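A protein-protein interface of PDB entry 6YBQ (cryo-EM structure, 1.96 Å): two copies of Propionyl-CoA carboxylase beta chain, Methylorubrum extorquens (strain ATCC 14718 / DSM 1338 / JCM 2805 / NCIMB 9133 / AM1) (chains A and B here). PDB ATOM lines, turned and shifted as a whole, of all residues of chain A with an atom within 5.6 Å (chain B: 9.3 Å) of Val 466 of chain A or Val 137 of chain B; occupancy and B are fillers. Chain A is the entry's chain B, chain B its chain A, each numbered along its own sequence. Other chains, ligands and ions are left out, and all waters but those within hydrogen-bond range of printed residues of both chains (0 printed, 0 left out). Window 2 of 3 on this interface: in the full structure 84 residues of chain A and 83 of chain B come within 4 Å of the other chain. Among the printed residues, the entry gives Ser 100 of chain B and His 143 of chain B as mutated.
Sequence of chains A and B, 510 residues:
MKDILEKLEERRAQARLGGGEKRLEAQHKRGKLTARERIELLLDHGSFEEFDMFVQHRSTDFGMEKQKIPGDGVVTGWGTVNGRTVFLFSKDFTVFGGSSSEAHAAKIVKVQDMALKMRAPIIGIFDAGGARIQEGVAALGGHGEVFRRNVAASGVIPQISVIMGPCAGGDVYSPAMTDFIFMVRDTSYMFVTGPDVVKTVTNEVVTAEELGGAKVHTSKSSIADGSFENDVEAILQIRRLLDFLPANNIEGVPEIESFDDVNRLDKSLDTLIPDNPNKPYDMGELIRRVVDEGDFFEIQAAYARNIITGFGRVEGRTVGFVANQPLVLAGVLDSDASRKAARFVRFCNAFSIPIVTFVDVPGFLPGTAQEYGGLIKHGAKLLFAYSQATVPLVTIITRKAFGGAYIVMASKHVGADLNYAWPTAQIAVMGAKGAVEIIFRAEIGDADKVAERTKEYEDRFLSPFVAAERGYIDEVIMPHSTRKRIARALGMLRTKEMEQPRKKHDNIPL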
ATOM      1  N   TYR A 406     -24.617  38.488   1.221  1.00  0.00           N
ATOM      2  CA  TYR A 406     -25.722  37.889   0.482  1.00  0.00           C
ATOM      3  C   TYR A 406     -26.545  36.979   1.379  1.00  0.00           C
ATOM      4  O   TYR A 406     -27.779  36.977   1.307  1.00  0.00           O
ATOM      5  CB  TYR A 406     -25.201  37.112  -0.731  1.00  0.00           C
ATOM      6  CG  TYR A 406     -26.068  35.941  -1.141  1.00  0.00           C
ATOM      7  CD1 TYR A 406     -27.245  36.134  -1.851  1.00  0.00           C
ATOM      8  CD2 TYR A 406     -25.707  34.646  -0.823  1.00  0.00           C
ATOM      9  CE1 TYR A 406     -28.032  35.070  -2.224  1.00  0.00           C
ATOM     10  CE2 TYR A 406     -26.485  33.578  -1.192  1.00  0.00           C
ATOM     11  CZ  TYR A 406     -27.645  33.792  -1.894  1.00  0.00           C
ATOM     12  OH  TYR A 406     -28.409  32.713  -2.246  1.00  0.00           O
ATOM     13  N   ILE A 427     -24.312  37.345  -8.216  1.00  0.00           N
ATOM     14  CA  ILE A 427     -24.406  36.540  -7.000  1.00  0.00           C
ATOM     15  C   ILE A 427     -23.202  35.601  -6.974  1.00  0.00           C
ATOM     16  O   ILE A 427     -23.129  34.657  -7.768  1.00  0.00           O
ATOM     17  CB  ILE A 427     -25.732  35.764  -6.949  1.00  0.00           C
ATOM     18  CG1 ILE A 427     -26.906  36.704  -7.250  1.00  0.00           C
ATOM     19  CG2 ILE A 427     -25.910  35.090  -5.603  1.00  0.00           C
ATOM     20  CD1 ILE A 427     -28.256  36.034  -7.320  1.00  0.00           C
ATOM     21  N   ALA A 428     -22.265  35.838  -6.053  1.00  0.00           N
ATOM     22  CA  ALA A 428     -20.987  35.131  -6.072  1.00  0.00           C
ATOM     23  C   ALA A 428     -20.311  35.194  -4.707  1.00  0.00           C
ATOM     24  O   ALA A 428     -20.651  36.020  -3.860  1.00  0.00           O
ATOM     25  CB  ALA A 428     -20.062  35.710  -7.145  1.00  0.00           C
ATOM     26  N   VAL A 429     -19.337  34.297  -4.514  1.00  0.00           N
ATOM     27  CA  VAL A 429     -18.586  34.246  -3.261  1.00  0.00           C
ATOM     28  C   VAL A 429     -17.771  35.517  -3.066  1.00  0.00           C
ATOM     29  O   VAL A 429     -17.607  35.996  -1.938  1.00  0.00           O
ATOM     30  CB  VAL A 429     -17.691  32.993  -3.212  1.00  0.00           C
ATOM     31  CG1 VAL A 429     -18.541  31.748  -3.177  1.00  0.00           C
ATOM     32  CG2 VAL A 429     -16.720  32.954  -4.390  1.00  0.00           C
ATOM     33  N   ARG A 460     -18.312  33.535 -16.312  1.00  0.00           N
ATOM     34  CA  ARG A 460     -18.887  32.273 -15.872  1.00  0.00           C
ATOM     35  C   ARG A 460     -19.641  32.352 -14.549  1.00  0.00           C
ATOM     36  O   ARG A 460     -20.543  31.537 -14.327  1.00  0.00           O
ATOM     37  CB  ARG A 460     -17.778  31.226 -15.759  1.00  0.00           C
ATOM     38  CG  ARG A 460     -18.260  29.854 -15.403  1.00  0.00           C
ATOM     39  CD  ARG A 460     -17.209  28.818 -15.737  1.00  0.00           C
ATOM     40  NE  ARG A 460     -17.568  27.502 -15.219  1.00  0.00           N
ATOM     41  CZ  ARG A 460     -16.697  26.589 -14.803  1.00  0.00           C
ATOM     42  NH1 ARG A 460     -17.138  25.427 -14.348  1.00  0.00           N
ATOM     43  NH2 ARG A 460     -15.393  26.829 -14.836  1.00  0.00           N
ATOM     44  N   PHE A 461     -19.314  33.300 -13.665  1.00  0.00           N
ATOM     45  CA  PHE A 461     -19.827  33.280 -12.296  1.00  0.00           C
ATOM     46  C   PHE A 461     -20.427  34.590 -11.794  1.00  0.00           C
ATOM     47  O   PHE A 461     -21.136  34.556 -10.783  1.00  0.00           O
ATOM     48  CB  PHE A 461     -18.717  32.864 -11.320  1.00  0.00           C
ATOM     49  CG  PHE A 461     -18.187  31.477 -11.551  1.00  0.00           C
ATOM     50  CD1 PHE A 461     -19.011  30.373 -11.433  1.00  0.00           C
ATOM     51  CD2 PHE A 461     -16.859  31.275 -11.872  1.00  0.00           C
ATOM     52  CE1 PHE A 461     -18.521  29.104 -11.640  1.00  0.00           C
ATOM     53  CE2 PHE A 461     -16.369  30.003 -12.080  1.00  0.00           C
ATOM     54  CZ  PHE A 461     -17.200  28.921 -11.962  1.00  0.00           C
ATOM     55  N   SER A 463     -23.064  36.691 -12.341  1.00  0.00           N
ATOM     56  CA  SER A 463     -24.348  36.704 -13.034  1.00  0.00           C
ATOM     57  C   SER A 463     -25.388  36.013 -12.156  1.00  0.00           C
ATOM     58  O   SER A 463     -25.029  35.420 -11.131  1.00  0.00           O
ATOM     59  CB  SER A 463     -24.231  36.014 -14.393  1.00  0.00           C
ATOM     60  OG  SER A 463     -23.746  34.695 -14.251  1.00  0.00           O
ATOM     61  N   PRO A 464     -26.675  36.069 -12.500  1.00  0.00           N
ATOM     62  CA  PRO A 464     -27.699  35.421 -11.667  1.00  0.00           C
ATOM     63  C   PRO A 464     -27.964  33.952 -11.963  1.00  0.00           C
ATOM     64  O   PRO A 464     -28.793  33.353 -11.269  1.00  0.00           O
ATOM     65  CB  PRO A 464     -28.952  36.255 -11.977  1.00  0.00           C
ATOM     66  CG  PRO A 464     -28.745  36.770 -13.332  1.00  0.00           C
ATOM     67  CD  PRO A 464     -27.277  36.927 -13.537  1.00  0.00           C
ATOM     68  N   PHE A 465     -27.293  33.352 -12.943  1.00  0.00           N
ATOM     69  CA  PHE A 465     -27.751  32.083 -13.496  1.00  0.00           C
ATOM     70  C   PHE A 465     -27.212  30.853 -12.770  1.00  0.00           C
ATOM     71  O   PHE A 465     -27.868  29.809 -12.794  1.00  0.00           O
ATOM     72  CB  PHE A 465     -27.405  32.015 -14.984  1.00  0.00           C
ATOM     73  CG  PHE A 465     -28.004  33.136 -15.787  1.00  0.00           C
ATOM     74  CD1 PHE A 465     -29.377  33.264 -15.900  1.00  0.00           C
ATOM     75  CD2 PHE A 465     -27.199  34.062 -16.415  1.00  0.00           C
ATOM     76  CE1 PHE A 465     -29.933  34.296 -16.629  1.00  0.00           C
ATOM     77  CE2 PHE A 465     -27.749  35.093 -17.146  1.00  0.00           C
ATOM     78  CZ  PHE A 465     -29.119  35.210 -17.251  1.00  0.00           C
ATOM     79  N   VAL A 466     -26.054  30.929 -12.114  1.00  0.00           N
ATOM     80  CA  VAL A 466     -25.629  29.800 -11.290  1.00  0.00           C
ATOM     81  C   VAL A 466     -26.554  29.645 -10.090  1.00  0.00           C
ATOM     82  O   VAL A 466     -26.941  28.529  -9.726  1.00  0.00           O
ATOM     83  CB  VAL A 466     -24.159  29.953 -10.855  1.00  0.00           C
ATOM     84  CG1 VAL A 466     -23.798  28.866  -9.863  1.00  0.00           C
ATOM     85  CG2 VAL A 466     -23.239  29.881 -12.050  1.00  0.00           C
ATOM     86  N   ALA A 467     -26.912  30.757  -9.447  1.00  0.00           N
ATOM     87  CA  ALA A 467     -27.889  30.701  -8.365  1.00  0.00           C
ATOM     88  C   ALA A 467     -29.228  30.166  -8.862  1.00  0.00           C
ATOM     89  O   ALA A 467     -29.880  29.371  -8.177  1.00  0.00           O
ATOM     90  CB  ALA A 467     -28.053  32.082  -7.737  1.00  0.00           C
ATOM     91  N   ALA A 468     -29.653  30.585 -10.055  1.00  0.00           N
ATOM     92  CA  ALA A 468     -30.908  30.088 -10.610  1.00  0.00           C
ATOM     93  C   ALA A 468     -30.842  28.587 -10.879  1.00  0.00           C
ATOM     94  O   ALA A 468     -31.807  27.861 -10.614  1.00  0.00           O
ATOM     95  CB  ALA A 468     -31.260  30.853 -11.883  1.00  0.00           C
ATOM     96  N   GLU A 469     -29.705  28.101 -11.385  1.00  0.00           N
ATOM     97  CA  GLU A 469     -29.579  26.683 -11.708  1.00  0.00           C
ATOM     98  C   GLU A 469     -29.743  25.808 -10.473  1.00  0.00           C
ATOM     99  O   GLU A 469     -30.273  24.696 -10.568  1.00  0.00           O
ATOM    100  CB  GLU A 469     -28.229  26.415 -12.376  1.00  0.00           C
ATOM    101  CG  GLU A 469     -28.138  26.871 -13.822  1.00  0.00           C
ATOM    102  CD  GLU A 469     -26.709  27.003 -14.308  1.00  0.00           C
ATOM    103  OE1 GLU A 469     -25.808  26.403 -13.684  1.00  0.00           O
ATOM    104  OE2 GLU A 469     -26.485  27.706 -15.315  1.00  0.00           O
ATOM    105  N   ARG A 470     -29.303  26.287  -9.313  1.00  0.00           N
ATOM    106  CA  ARG A 470     -29.462  25.582  -8.050  1.00  0.00           C
ATOM    107  C   ARG A 470     -30.798  25.861  -7.370  1.00  0.00           C
ATOM    108  O   ARG A 470     -31.049  25.324  -6.288  1.00  0.00           O
ATOM    109  CB  ARG A 470     -28.322  25.954  -7.098  1.00  0.00           C
ATOM    110  CG  ARG A 470     -26.935  25.528  -7.565  1.00  0.00           C
ATOM    111  CD  ARG A 470     -26.822  24.031  -7.731  1.00  0.00           C
ATOM    112  NE  ARG A 470     -27.102  23.321  -6.485  1.00  0.00           N
ATOM    113  CZ  ARG A 470     -26.182  22.752  -5.711  1.00  0.00           C
ATOM    114  NH1 ARG A 470     -24.897  22.785  -6.036  1.00  0.00           N
ATOM    115  NH2 ARG A 470     -26.557  22.136  -4.603  1.00  0.00           N
ATOM    116  N   GLY A 471     -31.659  26.670  -7.977  1.00  0.00           N
ATOM    117  CA  GLY A 471     -32.921  27.019  -7.359  1.00  0.00           C
ATOM    118  C   GLY A 471     -32.828  27.892  -6.129  1.00  0.00           C
ATOM    119  O   GLY A 471     -33.732  27.863  -5.293  1.00  0.00           O
ATOM    120  N   TYR A 472     -31.757  28.673  -5.989  1.00  0.00           N
ATOM    121  CA  TYR A 472     -31.670  29.657  -4.916  1.00  0.00           C
ATOM    122  C   TYR A 472     -32.450  30.927  -5.231  1.00  0.00           C
ATOM    123  O   TYR A 472     -32.848  31.643  -4.306  1.00  0.00           O
ATOM    124  CB  TYR A 472     -30.208  30.009  -4.639  1.00  0.00           C
ATOM    125  CG  TYR A 472     -29.349  28.850  -4.189  1.00  0.00           C
ATOM    126  CD1 TYR A 472     -29.909  27.689  -3.678  1.00  0.00           C
ATOM    127  CD2 TYR A 472     -27.970  28.923  -4.271  1.00  0.00           C
ATOM    128  CE1 TYR A 472     -29.124  26.643  -3.271  1.00  0.00           C
ATOM    129  CE2 TYR A 472     -27.180  27.882  -3.868  1.00  0.00           C
ATOM    130  CZ  TYR A 472     -27.760  26.744  -3.367  1.00  0.00           C
ATOM    131  OH  TYR A 472     -26.975  25.697  -2.959  1.00  0.00           O
ATOM    132  N   ASP B  61     -15.333  21.503 -10.311  1.00  0.00           N
ATOM    133  CA  ASP B  61     -14.705  22.724 -10.793  1.00  0.00           C
ATOM    134  C   ASP B  61     -13.280  22.851 -10.267  1.00  0.00           C
ATOM    135  O   ASP B  61     -13.007  22.568  -9.098  1.00  0.00           O
ATOM    136  CB  ASP B  61     -15.519  23.948 -10.371  1.00  0.00           C
ATOM    137  CG  ASP B  61     -16.774  24.133 -11.200  1.00  0.00           C
ATOM    138  OD1 ASP B  61     -16.691  24.029 -12.441  1.00  0.00           O
ATOM    139  OD2 ASP B  61     -17.843  24.385 -10.608  1.00  0.00           O
ATOM    140  N   SER B 100     -15.605  25.219   4.529  1.00  0.00           N
ATOM    141  CA  SER B 100     -16.984  24.747   4.514  1.00  0.00           C
ATOM    142  C   SER B 100     -17.462  24.527   3.085  1.00  0.00           C
ATOM    143  O   SER B 100     -17.369  25.427   2.245  1.00  0.00           O
ATOM    144  CB  SER B 100     -17.902  25.745   5.221  1.00  0.00           C
ATOM    145  OG  SER B 100     -19.251  25.317   5.173  1.00  0.00           O
ATOM    146  N   SER B 101     -17.981  23.337   2.824  1.00  0.00           N
ATOM    147  CA  SER B 101     -18.564  22.955   1.547  1.00  0.00           C
ATOM    148  C   SER B 101     -19.971  22.403   1.775  1.00  0.00           C
ATOM    149  O   SER B 101     -20.461  22.329   2.903  1.00  0.00           O
ATOM    150  CB  SER B 101     -17.672  21.935   0.836  1.00  0.00           C
ATOM    151  OG  SER B 101     -17.751  20.660   1.448  1.00  0.00           O
ATOM    152  N   GLU B 102     -20.615  22.000   0.678  1.00  0.00           N
ATOM    153  CA  GLU B 102     -22.014  21.580   0.734  1.00  0.00           C
ATOM    154  C   GLU B 102     -22.193  20.350   1.624  1.00  0.00           C
ATOM    155  O   GLU B 102     -23.021  20.348   2.545  1.00  0.00           O
ATOM    156  CB  GLU B 102     -22.517  21.324  -0.689  1.00  0.00           C
ATOM    157  CG  GLU B 102     -23.960  20.877  -0.790  1.00  0.00           C
ATOM    158  CD  GLU B 102     -24.486  20.915  -2.212  1.00  0.00           C
ATOM    159  OE1 GLU B 102     -23.750  21.376  -3.110  1.00  0.00           O
ATOM    160  OE2 GLU B 102     -25.637  20.485  -2.433  1.00  0.00           O
ATOM    161  N   ALA B 131     -15.873  29.679   3.901  1.00  0.00           N
ATOM    162  CA  ALA B 131     -16.444  29.030   2.727  1.00  0.00           C
ATOM    163  C   ALA B 131     -15.346  28.574   1.773  1.00  0.00           C
ATOM    164  O   ALA B 131     -14.323  29.243   1.607  1.00  0.00           O
ATOM    165  CB  ALA B 131     -17.395  29.987   2.009  1.00  0.00           C
ATOM    166  N   ARG B 132     -15.568  27.425   1.138  1.00  0.00           N
ATOM    167  CA  ARG B 132     -14.610  26.861   0.190  1.00  0.00           C
ATOM    168  C   ARG B 132     -14.818  27.516  -1.171  1.00  0.00           C
ATOM    169  O   ARG B 132     -15.859  27.330  -1.808  1.00  0.00           O
ATOM    170  CB  ARG B 132     -14.767  25.345   0.109  1.00  0.00           C
ATOM    171  CG  ARG B 132     -13.661  24.662  -0.665  1.00  0.00           C
ATOM    172  CD  ARG B 132     -13.799  23.150  -0.660  1.00  0.00           C
ATOM    173  NE  ARG B 132     -13.759  22.584   0.682  1.00  0.00           N
ATOM    174  CZ  ARG B 132     -14.154  21.356   0.993  1.00  0.00           C
ATOM    175  NH1 ARG B 132     -14.618  20.540   0.059  1.00  0.00           N
ATOM    176  NH2 ARG B 132     -14.080  20.939   2.245  1.00  0.00           N
ATOM    177  N   ILE B 133     -13.818  28.273  -1.622  1.00  0.00           N
ATOM    178  CA  ILE B 133     -13.993  29.150  -2.777  1.00  0.00           C
ATOM    179  C   ILE B 133     -14.277  28.343  -4.042  1.00  0.00           C
ATOM    180  O   ILE B 133     -15.133  28.716  -4.854  1.00  0.00           O
ATOM    181  CB  ILE B 133     -12.755  30.051  -2.941  1.00  0.00           C
ATOM    182  CG1 ILE B 133     -12.579  30.953  -1.713  1.00  0.00           C
ATOM    183  CG2 ILE B 133     -12.857  30.876  -4.201  1.00  0.00           C
ATOM    184  CD1 ILE B 133     -13.619  32.050  -1.571  1.00  0.00           C
ATOM    185  N   GLN B 134     -13.575  27.223  -4.225  1.00  0.00           N
ATOM    186  CA  GLN B 134     -13.715  26.448  -5.457  1.00  0.00           C
ATOM    187  C   GLN B 134     -15.156  26.015  -5.701  1.00  0.00           C
ATOM    188  O   GLN B 134     -15.552  25.811  -6.854  1.00  0.00           O
ATOM    189  CB  GLN B 134     -12.801  25.223  -5.420  1.00  0.00           C
ATOM    190  CG  GLN B 134     -11.321  25.540  -5.414  1.00  0.00           C
ATOM    191  CD  GLN B 134     -10.801  25.898  -4.043  1.00  0.00           C
ATOM    192  OE1 GLN B 134     -11.563  26.272  -3.153  1.00  0.00           O
ATOM    193  NE2 GLN B 134      -9.495  25.779  -3.860  1.00  0.00           N
ATOM    194  N   GLU B 135     -15.950  25.869  -4.645  1.00  0.00           N
ATOM    195  CA  GLU B 135     -17.327  25.416  -4.773  1.00  0.00           C
ATOM    196  C   GLU B 135     -18.314  26.547  -5.026  1.00  0.00           C
ATOM    197  O   GLU B 135     -19.451  26.277  -5.429  1.00  0.00           O
ATOM    198  CB  GLU B 135     -17.740  24.641  -3.519  1.00  0.00           C
ATOM    199  CG  GLU B 135     -17.104  23.263  -3.423  1.00  0.00           C
ATOM    200  CD  GLU B 135     -17.974  22.251  -2.700  1.00  0.00           C
ATOM    201  OE1 GLU B 135     -19.039  22.635  -2.174  1.00  0.00           O
ATOM    202  OE2 GLU B 135     -17.590  21.064  -2.658  1.00  0.00           O
ATOM    203  N   GLY B 136     -17.916  27.796  -4.807  1.00  0.00           N
ATOM    204  CA  GLY B 136     -18.777  28.900  -5.163  1.00  0.00           C
ATOM    205  C   GLY B 136     -20.011  29.032  -4.281  1.00  0.00           C
ATOM    206  O   GLY B 136     -20.025  28.655  -3.103  1.00  0.00           O
ATOM    207  N   VAL B 137     -21.076  29.566  -4.885  1.00  0.00           N
ATOM    208  CA  VAL B 137     -22.251  29.987  -4.126  1.00  0.00           C
ATOM    209  C   VAL B 137     -22.872  28.826  -3.361  1.00  0.00           C
ATOM    210  O   VAL B 137     -23.461  29.029  -2.293  1.00  0.00           O
ATOM    211  CB  VAL B 137     -23.270  30.669  -5.062  1.00  0.00           C
ATOM    212  CG1 VAL B 137     -23.773  29.715  -6.133  1.00  0.00           C
ATOM    213  CG2 VAL B 137     -24.432  31.215  -4.265  1.00  0.00           C
ATOM    214  N   ALA B 138     -22.747  27.599  -3.872  1.00  0.00           N
ATOM    215  CA  ALA B 138     -23.258  26.445  -3.142  1.00  0.00           C
ATOM    216  C   ALA B 138     -22.797  26.481  -1.690  1.00  0.00           C
ATOM    217  O   ALA B 138     -23.605  26.350  -0.763  1.00  0.00           O
ATOM    218  CB  ALA B 138     -22.815  25.151  -3.821  1.00  0.00           C
ATOM    219  N   ALA B 139     -21.501  26.713  -1.477  1.00  0.00           N
ATOM    220  CA  ALA B 139     -20.969  26.724  -0.120  1.00  0.00           C
ATOM    221  C   ALA B 139     -21.710  27.728   0.752  1.00  0.00           C
ATOM    222  O   ALA B 139     -22.080  27.418   1.893  1.00  0.00           O
ATOM    223  CB  ALA B 139     -19.474  27.032  -0.147  1.00  0.00           C
ATOM    224  N   LEU B 140     -21.962  28.927   0.225  1.00  0.00           N
ATOM    225  CA  LEU B 140     -22.700  29.930   0.985  1.00  0.00           C
ATOM    226  C   LEU B 140     -24.038  29.375   1.452  1.00  0.00           C
ATOM    227  O   LEU B 140     -24.403  29.504   2.628  1.00  0.00           O
ATOM    228  CB  LEU B 140     -22.902  31.189   0.143  1.00  0.00           C
ATOM    229  CG  LEU B 140     -21.654  31.832  -0.457  1.00  0.00           C
ATOM    230  CD1 LEU B 140     -22.046  33.005  -1.340  1.00  0.00           C
ATOM    231  CD2 LEU B 140     -20.680  32.273   0.617  1.00  0.00           C
ATOM    232  N   GLY B 141     -24.771  28.728   0.546  1.00  0.00           N
ATOM    233  CA  GLY B 141     -26.025  28.112   0.943  1.00  0.00           C
ATOM    234  C   GLY B 141     -25.865  27.271   2.189  1.00  0.00           C
ATOM    235  O   GLY B 141     -26.622  27.412   3.154  1.00  0.00           O
ATOM    236  N   GLY B 142     -24.837  26.424   2.206  1.00  0.00           N
ATOM    237  CA  GLY B 142     -24.600  25.596   3.371  1.00  0.00           C
ATOM    238  C   GLY B 142     -24.561  26.408   4.649  1.00  0.00           C
ATOM    239  O   GLY B 142     -25.314  26.138   5.590  1.00  0.00           O
ATOM    240  N   HIS B 143     -23.722  27.390   4.658  1.00  0.00           N
ATOM    241  CA  HIS B 143     -23.622  28.293   5.825  1.00  0.00           C
ATOM    242  C   HIS B 143     -25.030  28.767   6.290  1.00  0.00           C
ATOM    243  O   HIS B 143     -25.437  28.566   7.454  1.00  0.00           O
ATOM    244  CB  HIS B 143     -22.715  29.432   5.456  1.00  0.00           C
ATOM    245  CG  HIS B 143     -21.305  29.222   5.828  1.00  0.00           C
ATOM    246  ND1 HIS B 143     -20.294  29.688   5.091  1.00  0.00           N
ATOM    247  CD2 HIS B 143     -20.725  28.642   6.863  1.00  0.00           C
ATOM    248  CE1 HIS B 143     -19.159  29.432   5.657  1.00  0.00           C
ATOM    249  NE2 HIS B 143     -19.397  28.795   6.725  1.00  0.00           N
ATOM    250  N   GLY B 144     -25.862  29.236   5.344  1.00  0.00           N
ATOM    251  CA  GLY B 144     -27.192  29.696   5.688  1.00  0.00           C
ATOM    252  C   GLY B 144     -27.977  28.652   6.450  1.00  0.00           C
ATOM    253  O   GLY B 144     -28.518  28.930   7.524  1.00  0.00           O
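The side-chain carboxylate (OD1) of Asp 61 of chain B is in salt-bridge range of the guanidinium group (NH1) of Arg 460 of chain A. The side-chain carboxylate (OE2) of Glu 102 of chain B lies within salt-bridge range of the guanidinium group (NH2) of Arg 470 of chain A (2.9 Å).
OE1 of Glu 135 of chain B lies within hydrogen-bond range of N of Glu 102 of chain B (3.3 Å). O of Ala 467 of chain A is in hydrogen-bond range of N of Tyr 472 of chain A (3.0 Å).
Val 429 of chain A touches Gly 136 of chain B. Val 137 of chain B touches Val 429 of chain A. Val 466 of chain A touches Val 137 of chain B. CB of Ala 138 of chain B touches NH1 of Arg 470 of chain A, 3.9 Å away. Tyr 472 of chain A touches Ala 138 of chain B.
Val 466 of chain A touches just one residue of chain B: Val 137 (3.8 Å). Of chain A, only Val 429 and Val 466 come within 4 Å of Val 137 of chain B. No residue of chain B comes within 4 Å of Ala 467 of chain A. No residue of chain B comes within 4 Å of Ala 468 of chain A. No residue of chain B comes within 4 Å of Glu 469 of chain A. Of the printed residues of chain B, Arg 460 of chain A touches Asp 61 (2.4 Å). Printed residues of chain A within 4 Å of Glu 102 of chain B: Arg 470.
Printed residues of chain B that touch a printed residue of chain A: Asp 61, Glu 102, Gly 136, Val 137 and Ala 138. Hydrophobic or aromatic side chains of chain B within 4 Å of the printed part of chain A: Val 137 and Ala 138. Among the printed residues, Asp or Glu carboxylates within 4 Å of a Lys or Arg side-chain nitrogen of the other chain: Arg 460 of chain A with Asp 61 of chain B and Arg 470 of chain A with Glu 102 of chain B.
No position is printed for both chains.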
